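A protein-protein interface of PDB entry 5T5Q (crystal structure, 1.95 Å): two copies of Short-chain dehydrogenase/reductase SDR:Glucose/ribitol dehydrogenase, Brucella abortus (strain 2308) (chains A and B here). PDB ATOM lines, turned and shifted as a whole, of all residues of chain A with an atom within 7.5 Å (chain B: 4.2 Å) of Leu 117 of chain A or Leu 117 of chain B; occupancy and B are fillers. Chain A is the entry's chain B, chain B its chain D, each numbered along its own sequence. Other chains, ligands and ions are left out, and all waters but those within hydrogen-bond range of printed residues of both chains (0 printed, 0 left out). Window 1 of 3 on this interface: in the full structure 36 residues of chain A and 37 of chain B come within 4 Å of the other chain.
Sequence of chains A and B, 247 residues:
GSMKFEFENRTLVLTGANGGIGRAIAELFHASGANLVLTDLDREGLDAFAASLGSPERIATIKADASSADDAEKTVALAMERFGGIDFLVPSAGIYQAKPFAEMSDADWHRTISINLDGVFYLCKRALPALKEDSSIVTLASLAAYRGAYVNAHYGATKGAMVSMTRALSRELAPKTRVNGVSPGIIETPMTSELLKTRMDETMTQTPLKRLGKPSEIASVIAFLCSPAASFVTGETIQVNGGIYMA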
ATOM      1  N   ALA A  66      23.977 -17.616 -32.331  1.00  0.00           N
ATOM      2  CA  ALA A  66      24.803 -17.604 -31.128  1.00  0.00           C
ATOM      3  C   ALA A  66      24.749 -18.934 -30.384  1.00  0.00           C
ATOM      4  O   ALA A  66      25.696 -19.281 -29.672  1.00  0.00           O
ATOM      5  CB  ALA A  66      24.385 -16.453 -30.212  1.00  0.00           C
ATOM      6  N   ALA A  93      25.208 -11.088 -28.276  1.00  0.00           N
ATOM      7  CA  ALA A  93      23.910 -11.630 -28.669  1.00  0.00           C
ATOM      8  C   ALA A  93      23.158 -12.171 -27.459  1.00  0.00           C
ATOM      9  O   ALA A  93      23.708 -12.940 -26.666  1.00  0.00           O
ATOM     10  CB  ALA A  93      24.086 -12.740 -29.708  1.00  0.00           C
ATOM     11  N   GLY A  94      21.892 -11.781 -27.337  1.00  0.00           N
ATOM     12  CA  GLY A  94      21.055 -12.263 -26.256  1.00  0.00           C
ATOM     13  C   GLY A  94      19.603 -11.953 -26.541  1.00  0.00           C
ATOM     14  O   GLY A  94      19.288 -11.069 -27.343  1.00  0.00           O
ATOM     15  N   TRP A 109      12.633 -21.773 -21.157  1.00  0.00           N
ATOM     16  CA  TRP A 109      13.850 -21.775 -20.357  1.00  0.00           C
ATOM     17  C   TRP A 109      15.064 -22.096 -21.216  1.00  0.00           C
ATOM     18  O   TRP A 109      16.045 -21.339 -21.233  1.00  0.00           O
ATOM     19  CB  TRP A 109      13.731 -22.771 -19.205  1.00  0.00           C
ATOM     20  CG  TRP A 109      15.013 -22.936 -18.449  1.00  0.00           C
ATOM     21  CD1 TRP A 109      16.007 -23.838 -18.703  1.00  0.00           C
ATOM     22  CD2 TRP A 109      15.438 -22.182 -17.303  1.00  0.00           C
ATOM     23  NE1 TRP A 109      17.030 -23.683 -17.797  1.00  0.00           N
ATOM     24  CE2 TRP A 109      16.707 -22.674 -16.926  1.00  0.00           C
ATOM     25  CE3 TRP A 109      14.875 -21.132 -16.570  1.00  0.00           C
ATOM     26  CZ2 TRP A 109      17.427 -22.151 -15.842  1.00  0.00           C
ATOM     27  CZ3 TRP A 109      15.580 -20.620 -15.481  1.00  0.00           C
ATOM     28  CH2 TRP A 109      16.847 -21.132 -15.132  1.00  0.00           C
ATOM     29  N   ARG A 111      15.606 -22.014 -24.444  1.00  0.00           N
ATOM     30  CA  ARG A 111      15.974 -21.063 -25.488  1.00  0.00           C
ATOM     31  C   ARG A 111      16.792 -19.905 -24.923  1.00  0.00           C
ATOM     32  O   ARG A 111      17.771 -19.467 -25.542  1.00  0.00           O
ATOM     33  CB  ARG A 111      14.727 -20.548 -26.200  1.00  0.00           C
ATOM     34  CG  ARG A 111      15.068 -19.763 -27.429  1.00  0.00           C
ATOM     35  CD  ARG A 111      13.878 -19.574 -28.342  1.00  0.00           C
ATOM     36  NE  ARG A 111      13.857 -18.220 -28.890  1.00  0.00           N
ATOM     37  CZ  ARG A 111      14.589 -17.819 -29.927  1.00  0.00           C
ATOM     38  NH1 ARG A 111      14.504 -16.563 -30.347  1.00  0.00           N
ATOM     39  NH2 ARG A 111      15.408 -18.668 -30.536  1.00  0.00           N
ATOM     40  N   THR A 112      16.427 -19.408 -23.735  1.00  0.00           N
ATOM     41  CA  THR A 112      17.188 -18.298 -23.163  1.00  0.00           C
ATOM     42  C   THR A 112      18.555 -18.764 -22.669  1.00  0.00           C
ATOM     43  O   THR A 112      19.560 -18.059 -22.843  1.00  0.00           O
ATOM     44  CB  THR A 112      16.401 -17.615 -22.040  1.00  0.00           C
ATOM     45  OG1 THR A 112      15.391 -16.776 -22.610  1.00  0.00           O
ATOM     46  CG2 THR A 112      17.329 -16.731 -21.191  1.00  0.00           C
ATOM     47  N   ILE A 113      18.622 -19.938 -22.045  1.00  0.00           N
ATOM     48  CA  ILE A 113      19.920 -20.433 -21.602  1.00  0.00           C
ATOM     49  C   ILE A 113      20.813 -20.709 -22.811  1.00  0.00           C
ATOM     50  O   ILE A 113      22.007 -20.386 -22.807  1.00  0.00           O
ATOM     51  CB  ILE A 113      19.757 -21.680 -20.706  1.00  0.00           C
ATOM     52  CG1 ILE A 113      19.508 -21.302 -19.235  1.00  0.00           C
ATOM     53  CG2 ILE A 113      21.028 -22.542 -20.740  1.00  0.00           C
ATOM     54  CD1 ILE A 113      18.346 -20.338 -18.972  1.00  0.00           C
ATOM     55  N   SER A 114      20.243 -21.276 -23.876  1.00  0.00           N
ATOM     56  CA  SER A 114      21.053 -21.672 -25.022  1.00  0.00           C
ATOM     57  C   SER A 114      21.717 -20.465 -25.677  1.00  0.00           C
ATOM     58  O   SER A 114      22.917 -20.493 -25.984  1.00  0.00           O
ATOM     59  CB  SER A 114      20.199 -22.428 -26.037  1.00  0.00           C
ATOM     60  OG  SER A 114      20.997 -22.840 -27.133  1.00  0.00           O
ATOM     61  N   ILE A 115      20.952 -19.392 -25.900  1.00  0.00           N
ATOM     62  CA  ILE A 115      21.503 -18.208 -26.555  1.00  0.00           C
ATOM     63  C   ILE A 115      22.372 -17.398 -25.597  1.00  0.00           C
ATOM     64  O   ILE A 115      23.512 -17.052 -25.920  1.00  0.00           O
ATOM     65  CB  ILE A 115      20.371 -17.349 -27.145  1.00  0.00           C
ATOM     66  CG1 ILE A 115      19.677 -18.112 -28.284  1.00  0.00           C
ATOM     67  CG2 ILE A 115      20.899 -15.996 -27.616  1.00  0.00           C
ATOM     68  CD1 ILE A 115      18.405 -17.461 -28.755  1.00  0.00           C
ATOM     69  N   ASN A 116      21.849 -17.078 -24.407  1.00  0.00           N
ATOM     70  CA  ASN A 116      22.529 -16.141 -23.513  1.00  0.00           C
ATOM     71  C   ASN A 116      23.688 -16.765 -22.739  1.00  0.00           C
ATOM     72  O   ASN A 116      24.517 -16.020 -22.196  1.00  0.00           O
ATOM     73  CB  ASN A 116      21.563 -15.563 -22.480  1.00  0.00           C
ATOM     74  CG  ASN A 116      20.498 -14.685 -23.082  1.00  0.00           C
ATOM     75  OD1 ASN A 116      20.343 -14.609 -24.289  1.00  0.00           O
ATOM     76  ND2 ASN A 116      19.745 -14.017 -22.224  1.00  0.00           N
ATOM     77  N   LEU A 117      23.743 -18.095 -22.629  1.00  0.00           N
ATOM     78  CA  LEU A 117      24.775 -18.704 -21.794  1.00  0.00           C
ATOM     79  C   LEU A 117      25.603 -19.729 -22.562  1.00  0.00           C
ATOM     80  O   LEU A 117      26.820 -19.559 -22.679  1.00  0.00           O
ATOM     81  CB  LEU A 117      24.148 -19.335 -20.540  1.00  0.00           C
ATOM     82  CG  LEU A 117      25.093 -20.086 -19.586  1.00  0.00           C
ATOM     83  CD1 LEU A 117      26.316 -19.230 -19.215  1.00  0.00           C
ATOM     84  CD2 LEU A 117      24.345 -20.536 -18.326  1.00  0.00           C
ATOM     85  N   ASP A 118      24.978 -20.792 -23.080  1.00  0.00           N
ATOM     86  CA  ASP A 118      25.738 -21.755 -23.875  1.00  0.00           C
ATOM     87  C   ASP A 118      26.490 -21.048 -25.002  1.00  0.00           C
ATOM     88  O   ASP A 118      27.671 -21.330 -25.258  1.00  0.00           O
ATOM     89  CB  ASP A 118      24.818 -22.823 -24.473  1.00  0.00           C
ATOM     90  CG  ASP A 118      24.120 -23.682 -23.437  1.00  0.00           C
ATOM     91  OD1 ASP A 118      24.547 -23.736 -22.254  1.00  0.00           O
ATOM     92  OD2 ASP A 118      23.137 -24.353 -23.843  1.00  0.00           O
ATOM     93  N   GLY A 119      25.819 -20.116 -25.681  1.00  0.00           N
ATOM     94  CA  GLY A 119      26.457 -19.431 -26.792  1.00  0.00           C
ATOM     95  C   GLY A 119      27.706 -18.678 -26.374  1.00  0.00           C
ATOM     96  O   GLY A 119      28.694 -18.623 -27.119  1.00  0.00           O
ATOM     97  N   VAL A 120      27.680 -18.085 -25.180  1.00  0.00           N
ATOM     98  CA  VAL A 120      28.867 -17.397 -24.695  1.00  0.00           C
ATOM     99  C   VAL A 120      29.994 -18.395 -24.469  1.00  0.00           C
ATOM    100  O   VAL A 120      31.154 -18.134 -24.819  1.00  0.00           O
ATOM    101  CB  VAL A 120      28.531 -16.605 -23.423  1.00  0.00           C
ATOM    102  CG1 VAL A 120      29.784 -15.915 -22.892  1.00  0.00           C
ATOM    103  CG2 VAL A 120      27.441 -15.597 -23.731  1.00  0.00           C
ATOM    104  N   PHE A 121      29.677 -19.561 -23.895  1.00  0.00           N
ATOM    105  CA  PHE A 121      30.682 -20.617 -23.791  1.00  0.00           C
ATOM    106  C   PHE A 121      31.254 -20.977 -25.163  1.00  0.00           C
ATOM    107  O   PHE A 121      32.474 -21.081 -25.327  1.00  0.00           O
ATOM    108  CB  PHE A 121      30.107 -21.857 -23.122  1.00  0.00           C
ATOM    109  CG  PHE A 121      30.966 -23.075 -23.325  1.00  0.00           C
ATOM    110  CD1 PHE A 121      30.564 -24.091 -24.161  1.00  0.00           C
ATOM    111  CD2 PHE A 121      32.213 -23.162 -22.721  1.00  0.00           C
ATOM    112  CE1 PHE A 121      31.374 -25.203 -24.366  1.00  0.00           C
ATOM    113  CE2 PHE A 121      33.025 -24.274 -22.917  1.00  0.00           C
ATOM    114  CZ  PHE A 121      32.599 -25.292 -23.742  1.00  0.00           C
ATOM    115  N   TYR A 122      30.388 -21.204 -26.161  1.00  0.00           N
ATOM    116  CA  TYR A 122      30.886 -21.623 -27.471  1.00  0.00           C
ATOM    117  C   TYR A 122      31.857 -20.608 -28.050  1.00  0.00           C
ATOM    118  O   TYR A 122      32.942 -20.967 -28.523  1.00  0.00           O
ATOM    119  CB  TYR A 122      29.738 -21.848 -28.460  1.00  0.00           C
ATOM    120  CG  TYR A 122      28.818 -22.993 -28.118  1.00  0.00           C
ATOM    121  CD1 TYR A 122      29.292 -24.135 -27.486  1.00  0.00           C
ATOM    122  CD2 TYR A 122      27.477 -22.949 -28.480  1.00  0.00           C
ATOM    123  CE1 TYR A 122      28.443 -25.188 -27.192  1.00  0.00           C
ATOM    124  CE2 TYR A 122      26.633 -23.973 -28.192  1.00  0.00           C
ATOM    125  CZ  TYR A 122      27.110 -25.091 -27.553  1.00  0.00           C
ATOM    126  OH  TYR A 122      26.227 -26.100 -27.284  1.00  0.00           O
ATOM    127  N   LEU A 123      31.489 -19.327 -28.023  1.00  0.00           N
ATOM    128  CA  LEU A 123      32.351 -18.339 -28.660  1.00  0.00           C
ATOM    129  C   LEU A 123      33.668 -18.193 -27.903  1.00  0.00           C
ATOM    130  O   LEU A 123      34.745 -18.173 -28.514  1.00  0.00           O
ATOM    131  CB  LEU A 123      31.634 -16.990 -28.769  1.00  0.00           C
ATOM    132  CG  LEU A 123      32.366 -15.978 -29.663  1.00  0.00           C
ATOM    133  CD1 LEU A 123      32.309 -16.391 -31.126  1.00  0.00           C
ATOM    134  CD2 LEU A 123      31.838 -14.554 -29.496  1.00  0.00           C
ATOM    135  N   ALA A 153      12.957 -14.827 -15.038  1.00  0.00           N
ATOM    136  CA  ALA A 153      13.899 -15.560 -14.188  1.00  0.00           C
ATOM    137  C   ALA A 153      14.988 -16.241 -15.005  1.00  0.00           C
ATOM    138  O   ALA A 153      16.119 -16.380 -14.526  1.00  0.00           O
ATOM    139  CB  ALA A 153      13.181 -16.606 -13.341  1.00  0.00           C
ATOM    140  N   HIS A 154      14.663 -16.701 -16.217  1.00  0.00           N
ATOM    141  CA  HIS A 154      15.693 -17.308 -17.055  1.00  0.00           C
ATOM    142  C   HIS A 154      16.707 -16.263 -17.493  1.00  0.00           C
ATOM    143  O   HIS A 154      17.918 -16.495 -17.408  1.00  0.00           O
ATOM    144  CB  HIS A 154      15.076 -18.045 -18.258  1.00  0.00           C
ATOM    145  CG  HIS A 154      14.040 -17.273 -19.033  1.00  0.00           C
ATOM    146  ND1 HIS A 154      13.610 -16.005 -18.688  1.00  0.00           N
ATOM    147  CD2 HIS A 154      13.343 -17.610 -20.149  1.00  0.00           C
ATOM    148  CE1 HIS A 154      12.711 -15.591 -19.560  1.00  0.00           C
ATOM    149  NE2 HIS A 154      12.531 -16.546 -20.459  1.00  0.00           N
ATOM    150  N   ALA A 157      18.977 -15.404 -14.523  1.00  0.00           N
ATOM    151  CA  ALA A 157      19.925 -16.491 -14.330  1.00  0.00           C
ATOM    152  C   ALA A 157      21.100 -16.379 -15.299  1.00  0.00           C
ATOM    153  O   ALA A 157      22.263 -16.465 -14.884  1.00  0.00           O
ATOM    154  CB  ALA A 157      19.208 -17.832 -14.509  1.00  0.00           C
ATOM    155  N   THR A 158      20.821 -16.170 -16.600  1.00  0.00           N
ATOM    156  CA  THR A 158      21.930 -16.117 -17.553  1.00  0.00           C
ATOM    157  C   THR A 158      22.830 -14.911 -17.293  1.00  0.00           C
ATOM    158  O   THR A 158      24.047 -14.999 -17.482  1.00  0.00           O
ATOM    159  CB  THR A 158      21.439 -16.117 -19.015  1.00  0.00           C
ATOM    160  OG1 THR A 158      20.688 -14.929 -19.307  1.00  0.00           O
ATOM    161  CG2 THR A 158      20.578 -17.338 -19.312  1.00  0.00           C
ATOM    162  N   LYS A 159      22.266 -13.792 -16.835  1.00  0.00           N
ATOM    163  CA  LYS A 159      23.081 -12.607 -16.579  1.00  0.00           C
ATOM    164  C   LYS A 159      23.841 -12.700 -15.241  1.00  0.00           C
ATOM    165  O   LYS A 159      24.948 -12.164 -15.123  1.00  0.00           O
ATOM    166  CB  LYS A 159      22.187 -11.360 -16.684  1.00  0.00           C
ATOM    167  CG  LYS A 159      21.598 -11.158 -18.125  1.00  0.00           C
ATOM    168  CD  LYS A 159      22.694 -11.279 -19.190  1.00  0.00           C
ATOM    169  CE  LYS A 159      22.223 -10.842 -20.592  1.00  0.00           C
ATOM    170  NZ  LYS A 159      23.383 -10.827 -21.559  1.00  0.00           N
ATOM    171  N   GLY A 160      23.313 -13.397 -14.232  1.00  0.00           N
ATOM    172  CA  GLY A 160      24.158 -13.740 -13.090  1.00  0.00           C
ATOM    173  C   GLY A 160      25.285 -14.687 -13.476  1.00  0.00           C
ATOM    174  O   GLY A 160      26.416 -14.576 -12.984  1.00  0.00           O
ATOM    175  N   ALA A 161      24.991 -15.637 -14.363  1.00  0.00           N
ATOM    176  CA  ALA A 161      26.037 -16.515 -14.876  1.00  0.00           C
ATOM    177  C   ALA A 161      27.142 -15.727 -15.581  1.00  0.00           C
ATOM    178  O   ALA A 161      28.326 -16.043 -15.424  1.00  0.00           O
ATOM    179  CB  ALA A 161      25.429 -17.559 -15.824  1.00  0.00           C
ATOM    180  N   MET A 162      26.784 -14.702 -16.366  1.00  0.00           N
ATOM    181  CA  MET A 162      27.830 -13.892 -16.998  1.00  0.00           C
ATOM    182  C   MET A 162      28.795 -13.314 -15.956  1.00  0.00           C
ATOM    183  O   MET A 162      30.018 -13.348 -16.141  1.00  0.00           O
ATOM    184  CB  MET A 162      27.226 -12.756 -17.836  1.00  0.00           C
ATOM    185  CG  MET A 162      26.567 -13.199 -19.138  1.00  0.00           C
ATOM    186  SD  MET A 162      27.681 -14.136 -20.224  1.00  0.00           S
ATOM    187  CE  MET A 162      27.100 -15.804 -19.903  1.00  0.00           C
ATOM    188  N   MET A 165      30.940 -16.131 -14.610  1.00  0.00           N
ATOM    189  CA  MET A 165      31.779 -16.688 -15.672  1.00  0.00           C
ATOM    190  C   MET A 165      32.887 -15.723 -16.056  1.00  0.00           C
ATOM    191  O   MET A 165      34.010 -16.146 -16.367  1.00  0.00           O
ATOM    192  CB  MET A 165      30.925 -17.046 -16.881  1.00  0.00           C
ATOM    193  CG  MET A 165      31.691 -17.814 -17.951  1.00  0.00           C
ATOM    194  SD  MET A 165      30.522 -18.182 -19.258  1.00  0.00           S
ATOM    195  CE  MET A 165      31.596 -19.006 -20.452  1.00  0.00           C
ATOM    196  N   TRP B 109      30.590 -28.923 -20.681  1.00  0.00           N
ATOM    197  CA  TRP B 109      29.813 -27.731 -20.374  1.00  0.00           C
ATOM    198  C   TRP B 109      28.354 -28.089 -20.136  1.00  0.00           C
ATOM    199  O   TRP B 109      27.776 -27.751 -19.091  1.00  0.00           O
ATOM    200  CB  TRP B 109      29.944 -26.714 -21.515  1.00  0.00           C
ATOM    201  CG  TRP B 109      29.033 -25.532 -21.359  1.00  0.00           C
ATOM    202  CD1 TRP B 109      27.766 -25.415 -21.839  1.00  0.00           C
ATOM    203  CD2 TRP B 109      29.310 -24.305 -20.654  1.00  0.00           C
ATOM    204  NE1 TRP B 109      27.236 -24.202 -21.479  1.00  0.00           N
ATOM    205  CE2 TRP B 109      28.167 -23.495 -20.768  1.00  0.00           C
ATOM    206  CE3 TRP B 109      30.419 -23.811 -19.952  1.00  0.00           C
ATOM    207  CZ2 TRP B 109      28.092 -22.218 -20.201  1.00  0.00           C
ATOM    208  CZ3 TRP B 109      30.346 -22.533 -19.390  1.00  0.00           C
ATOM    209  CH2 TRP B 109      29.190 -21.756 -19.520  1.00  0.00           C
ATOM    210  N   ILE B 113      25.805 -27.529 -16.734  1.00  0.00           N
ATOM    211  CA  ILE B 113      24.650 -26.631 -16.810  1.00  0.00           C
ATOM    212  C   ILE B 113      23.345 -27.404 -16.611  1.00  0.00           C
ATOM    213  O   ILE B 113      22.432 -26.947 -15.909  1.00  0.00           O
ATOM    214  CB  ILE B 113      24.653 -25.850 -18.142  1.00  0.00           C
ATOM    215  CG1 ILE B 113      25.475 -24.556 -18.046  1.00  0.00           C
ATOM    216  CG2 ILE B 113      23.239 -25.479 -18.554  1.00  0.00           C
ATOM    217  CD1 ILE B 113      26.896 -24.724 -17.550  1.00  0.00           C
ATOM    218  N   SER B 114      23.242 -28.593 -17.201  1.00  0.00           N
ATOM    219  CA  SER B 114      21.997 -29.354 -17.121  1.00  0.00           C
ATOM    220  C   SER B 114      21.664 -29.723 -15.680  1.00  0.00           C
ATOM    221  O   SER B 114      20.522 -29.567 -15.231  1.00  0.00           O
ATOM    222  CB  SER B 114      22.099 -30.608 -17.989  1.00  0.00           C
ATOM    223  OG  SER B 114      20.848 -31.260 -18.078  1.00  0.00           O
ATOM    224  N   ILE B 115      22.653 -30.219 -14.938  1.00  0.00           N
ATOM    225  CA  ILE B 115      22.424 -30.656 -13.565  1.00  0.00           C
ATOM    226  C   ILE B 115      22.287 -29.464 -12.623  1.00  0.00           C
ATOM    227  O   ILE B 115      21.324 -29.367 -11.851  1.00  0.00           O
ATOM    228  CB  ILE B 115      23.563 -31.595 -13.126  1.00  0.00           C
ATOM    229  CG1 ILE B 115      23.522 -32.893 -13.964  1.00  0.00           C
ATOM    230  CG2 ILE B 115      23.507 -31.839 -11.627  1.00  0.00           C
ATOM    231  CD1 ILE B 115      24.736 -33.792 -13.799  1.00  0.00           C
ATOM    232  N   ASN B 116      23.245 -28.541 -12.680  1.00  0.00           N
ATOM    233  CA  ASN B 116      23.329 -27.447 -11.716  1.00  0.00           C
ATOM    234  C   ASN B 116      22.354 -26.318 -11.997  1.00  0.00           C
ATOM    235  O   ASN B 116      22.091 -25.517 -11.096  1.00  0.00           O
ATOM    236  CB  ASN B 116      24.746 -26.860 -11.695  1.00  0.00           C
ATOM    237  CG  ASN B 116      25.775 -27.816 -11.122  1.00  0.00           C
ATOM    238  OD1 ASN B 116      25.484 -28.985 -10.872  1.00  0.00           O
ATOM    239  ND2 ASN B 116      26.990 -27.325 -10.922  1.00  0.00           N
ATOM    240  N   LEU B 117      21.832 -26.208 -13.219  1.00  0.00           N
ATOM    241  CA  LEU B 117      21.018 -25.041 -13.530  1.00  0.00           C
ATOM    242  C   LEU B 117      19.657 -25.443 -14.074  1.00  0.00           C
ATOM    243  O   LEU B 117      18.634 -25.096 -13.476  1.00  0.00           O
ATOM    244  CB  LEU B 117      21.761 -24.114 -14.509  1.00  0.00           C
ATOM    245  CG  LEU B 117      21.071 -22.845 -15.035  1.00  0.00           C
ATOM    246  CD1 LEU B 117      20.505 -21.975 -13.904  1.00  0.00           C
ATOM    247  CD2 LEU B 117      22.047 -22.024 -15.859  1.00  0.00           C
ATOM    248  N   ASP B 118      19.627 -26.175 -15.204  1.00  0.00           N
ATOM    249  CA  ASP B 118      18.352 -26.640 -15.738  1.00  0.00           C
ATOM    250  C   ASP B 118      17.556 -27.390 -14.684  1.00  0.00           C
ATOM    251  O   ASP B 118      16.341 -27.188 -14.548  1.00  0.00           O
ATOM    252  CB  ASP B 118      18.562 -27.545 -16.961  1.00  0.00           C
ATOM    253  CG  ASP B 118      19.187 -26.812 -18.136  1.00  0.00           C
ATOM    254  OD1 ASP B 118      19.147 -25.560 -18.152  1.00  0.00           O
ATOM    255  OD2 ASP B 118      19.701 -27.487 -19.052  1.00  0.00           O
ATOM    256  N   GLY B 119      18.225 -28.271 -13.937  1.00  0.00           N
ATOM    257  CA  GLY B 119      17.521 -29.056 -12.937  1.00  0.00           C
ATOM    258  C   GLY B 119      16.869 -28.192 -11.880  1.00  0.00           C
ATOM    259  O   GLY B 119      15.742 -28.456 -11.449  1.00  0.00           O
ATOM    260  N   VAL B 120      17.546 -27.118 -11.483  1.00  0.00           N
ATOM    261  CA  VAL B 120      16.960 -26.221 -10.499  1.00  0.00           C
ATOM    262  C   VAL B 120      15.712 -25.559 -11.075  1.00  0.00           C
ATOM    263  O   VAL B 120      14.673 -25.473 -10.407  1.00  0.00           O
ATOM    264  CB  VAL B 120      18.011 -25.200 -10.024  1.00  0.00           C
ATOM    265  CG1 VAL B 120      17.401 -24.214  -9.054  1.00  0.00           C
ATOM    266  CG2 VAL B 120      19.176 -25.939  -9.361  1.00  0.00           C
ATOM    267  N   PHE B 121      15.767 -25.147 -12.346  1.00  0.00           N
ATOM    268  CA  PHE B 121      14.568 -24.623 -12.990  1.00  0.00           C
ATOM    269  C   PHE B 121      13.431 -25.629 -12.948  1.00  0.00           C
ATOM    270  O   PHE B 121      12.309 -25.283 -12.563  1.00  0.00           O
ATOM    271  CB  PHE B 121      14.822 -24.222 -14.439  1.00  0.00           C
ATOM    272  CG  PHE B 121      13.550 -24.079 -15.230  1.00  0.00           C
ATOM    273  CD1 PHE B 121      12.655 -23.064 -14.936  1.00  0.00           C
ATOM    274  CD2 PHE B 121      13.231 -24.971 -16.239  1.00  0.00           C
ATOM    275  CE1 PHE B 121      11.471 -22.934 -15.626  1.00  0.00           C
ATOM    276  CE2 PHE B 121      12.043 -24.845 -16.942  1.00  0.00           C
ATOM    277  CZ  PHE B 121      11.159 -23.825 -16.636  1.00  0.00           C
ATOM    278  N   THR B 158      27.097 -21.624 -13.337  1.00  0.00           N
ATOM    279  CA  THR B 158      25.838 -22.090 -12.764  1.00  0.00           C
ATOM    280  C   THR B 158      25.634 -21.553 -11.354  1.00  0.00           C
ATOM    281  O   THR B 158      24.495 -21.277 -10.962  1.00  0.00           O
ATOM    282  CB  THR B 158      25.758 -23.622 -12.760  1.00  0.00           C
ATOM    283  OG1 THR B 158      26.764 -24.174 -11.889  1.00  0.00           O
ATOM    284  CG2 THR B 158      25.926 -24.175 -14.187  1.00  0.00           C
ATOM    285  N   ALA B 161      24.483 -18.051 -11.675  1.00  0.00           N
ATOM    286  CA  ALA B 161      23.078 -18.149 -12.059  1.00  0.00           C
ATOM    287  C   ALA B 161      22.184 -18.380 -10.833  1.00  0.00           C
ATOM    288  O   ALA B 161      21.082 -17.832 -10.752  1.00  0.00           O
ATOM    289  CB  ALA B 161      22.890 -19.270 -13.086  1.00  0.00           C
ATOM    290  N   MET B 162      22.630 -19.203  -9.878  1.00  0.00           N
ATOM    291  CA  MET B 162      21.841 -19.416  -8.659  1.00  0.00           C
ATOM    292  C   MET B 162      21.577 -18.113  -7.913  1.00  0.00           C
ATOM    293  O   MET B 162      20.462 -17.885  -7.424  1.00  0.00           O
ATOM    294  CB  MET B 162      22.533 -20.419  -7.744  1.00  0.00           C
ATOM    295  CG  MET B 162      22.438 -21.868  -8.231  1.00  0.00           C
ATOM    296  SD  MET B 162      20.737 -22.471  -8.477  1.00  0.00           S
ATOM    297  CE  MET B 162      20.590 -22.367 -10.264  1.00  0.00           C
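The indole nitrogen (NE1) of Trp 109 of chain A lies within hydrogen-bond range of the side-chain carboxylate (OD1) of Asp 118 of chain B, 2.9 Å away. The indole nitrogen (NE1) of Trp 109 of chain B lies within hydrogen-bond range of the side-chain carboxylate (OD1) of Asp 118 of chain A (2.8 Å).
O of Ile 113 of chain A sits at hydrogen-bond distance from N of Asp 118 of chain A (3.0 Å). The backbone NH of Asp 118 of chain B is in hydrogen-bond range of the backbone carbonyl oxygen of Ile 113 of chain B, at 3.0 Å.
Trp 109 of chain A touches Leu 117 of chain B (CZ2 to CD1, 3.6 Å). CD1 of Phe 121 of chain B touches CE3 of Trp 109 of chain A, at 3.4 Å. Trp 109 of chain B touches Leu 117 of chain A. Leu 117 of chain B touches Leu 117 of chain A (CD2 to CD2, 3.7 Å). Phe 121 of chain A touches Trp 109 of chain B. Ala 157 of chain A touches Ala 161 of chain B. Ala 161 of chain B touches Gly 160 of chain A. N of Ala 161 of chain B touches N of Ala 161 of chain A, 3.6 Å away. Trp 109 of chain B touches Met 165 of chain A.
Of chain B, only Trp 109 and Leu 117 come within 4 Å of Leu 117 of chain A. Leu 117 of chain B touches just these residues of chain A: Trp 109 (3.6 Å) and Leu 117 (3.7 Å). Of the printed residues of chain B, Phe 121 of chain A touches Trp 109. Of the printed residues of chain B, Trp 109 of chain A touches Leu 117 (3.6 Å), Asp 118 (2.9 Å) and Phe 121 (3.4 Å). Printed residues of chain B within 4 Å of Ala 157 of chain A: Ala 161 (3.4 Å). Printed residues of chain B within 4 Å of Asp 118 of chain A: Trp 109. Asn 116 of chain B touches none of the printed residues of chain A. The nearest printed residue of chain B that does not touch Leu 117 of chain A is Ile 113 of chain B (4.2 Å). The nearest residue of chain A that does not touch Leu 117 of chain B is Ile 113 of chain A (4.3 Å).
Printed residues of chain A that touch a printed residue of chain B: Trp 109, Leu 117, Asp 118, Phe 121, Ala 157, Gly 160, Ala 161 and Met 165. Hydrophobic or aromatic side chains of chain A within 4 Å of the printed part of chain B: Trp 109, Leu 117, Phe 121 and Met 165. Of the 13 printed residues of chain B, 5 touch a printed residue of chain A. Printed residues of chain B that touch a printed residue of chain A: Trp 109, Leu 117, Asp 118, Phe 121 and Ala 161. Hydrophobic or aromatic side chains of chain B that line the printed part of chain A: Trp 109, Leu 117, Phe 121 and Ala 161. Among the printed residues, 11 pairs touch across the chains. Among the printed residues, no Asp or Glu carboxylate lies within 4 Å of a Lys or Arg side-chain nitrogen of the other chain.
Trp 109 of chain A touches Leu 117 of chain B, and with the chains exchanged Leu 117 of chain A touches Trp 109 of chain B. Trp 109 of chain A touches Asp 118 of chain B, and with the chains exchanged Asp 118 of chain A touches Trp 109 of chain B. Leu 117 of chain A touches its own counterpart, Leu 117 of chain B. Ala 161 of chain B touches its own counterpart, Ala 161 of chain A. Positions printed for both chains: 109, 113, 114, 115, 116, 117, 118, 119, 120, 121, 158, 161 and 162. Of the 11 pairs that touch across the chains among the printed residues, 8 have their exchanged pair printed and touching as well.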
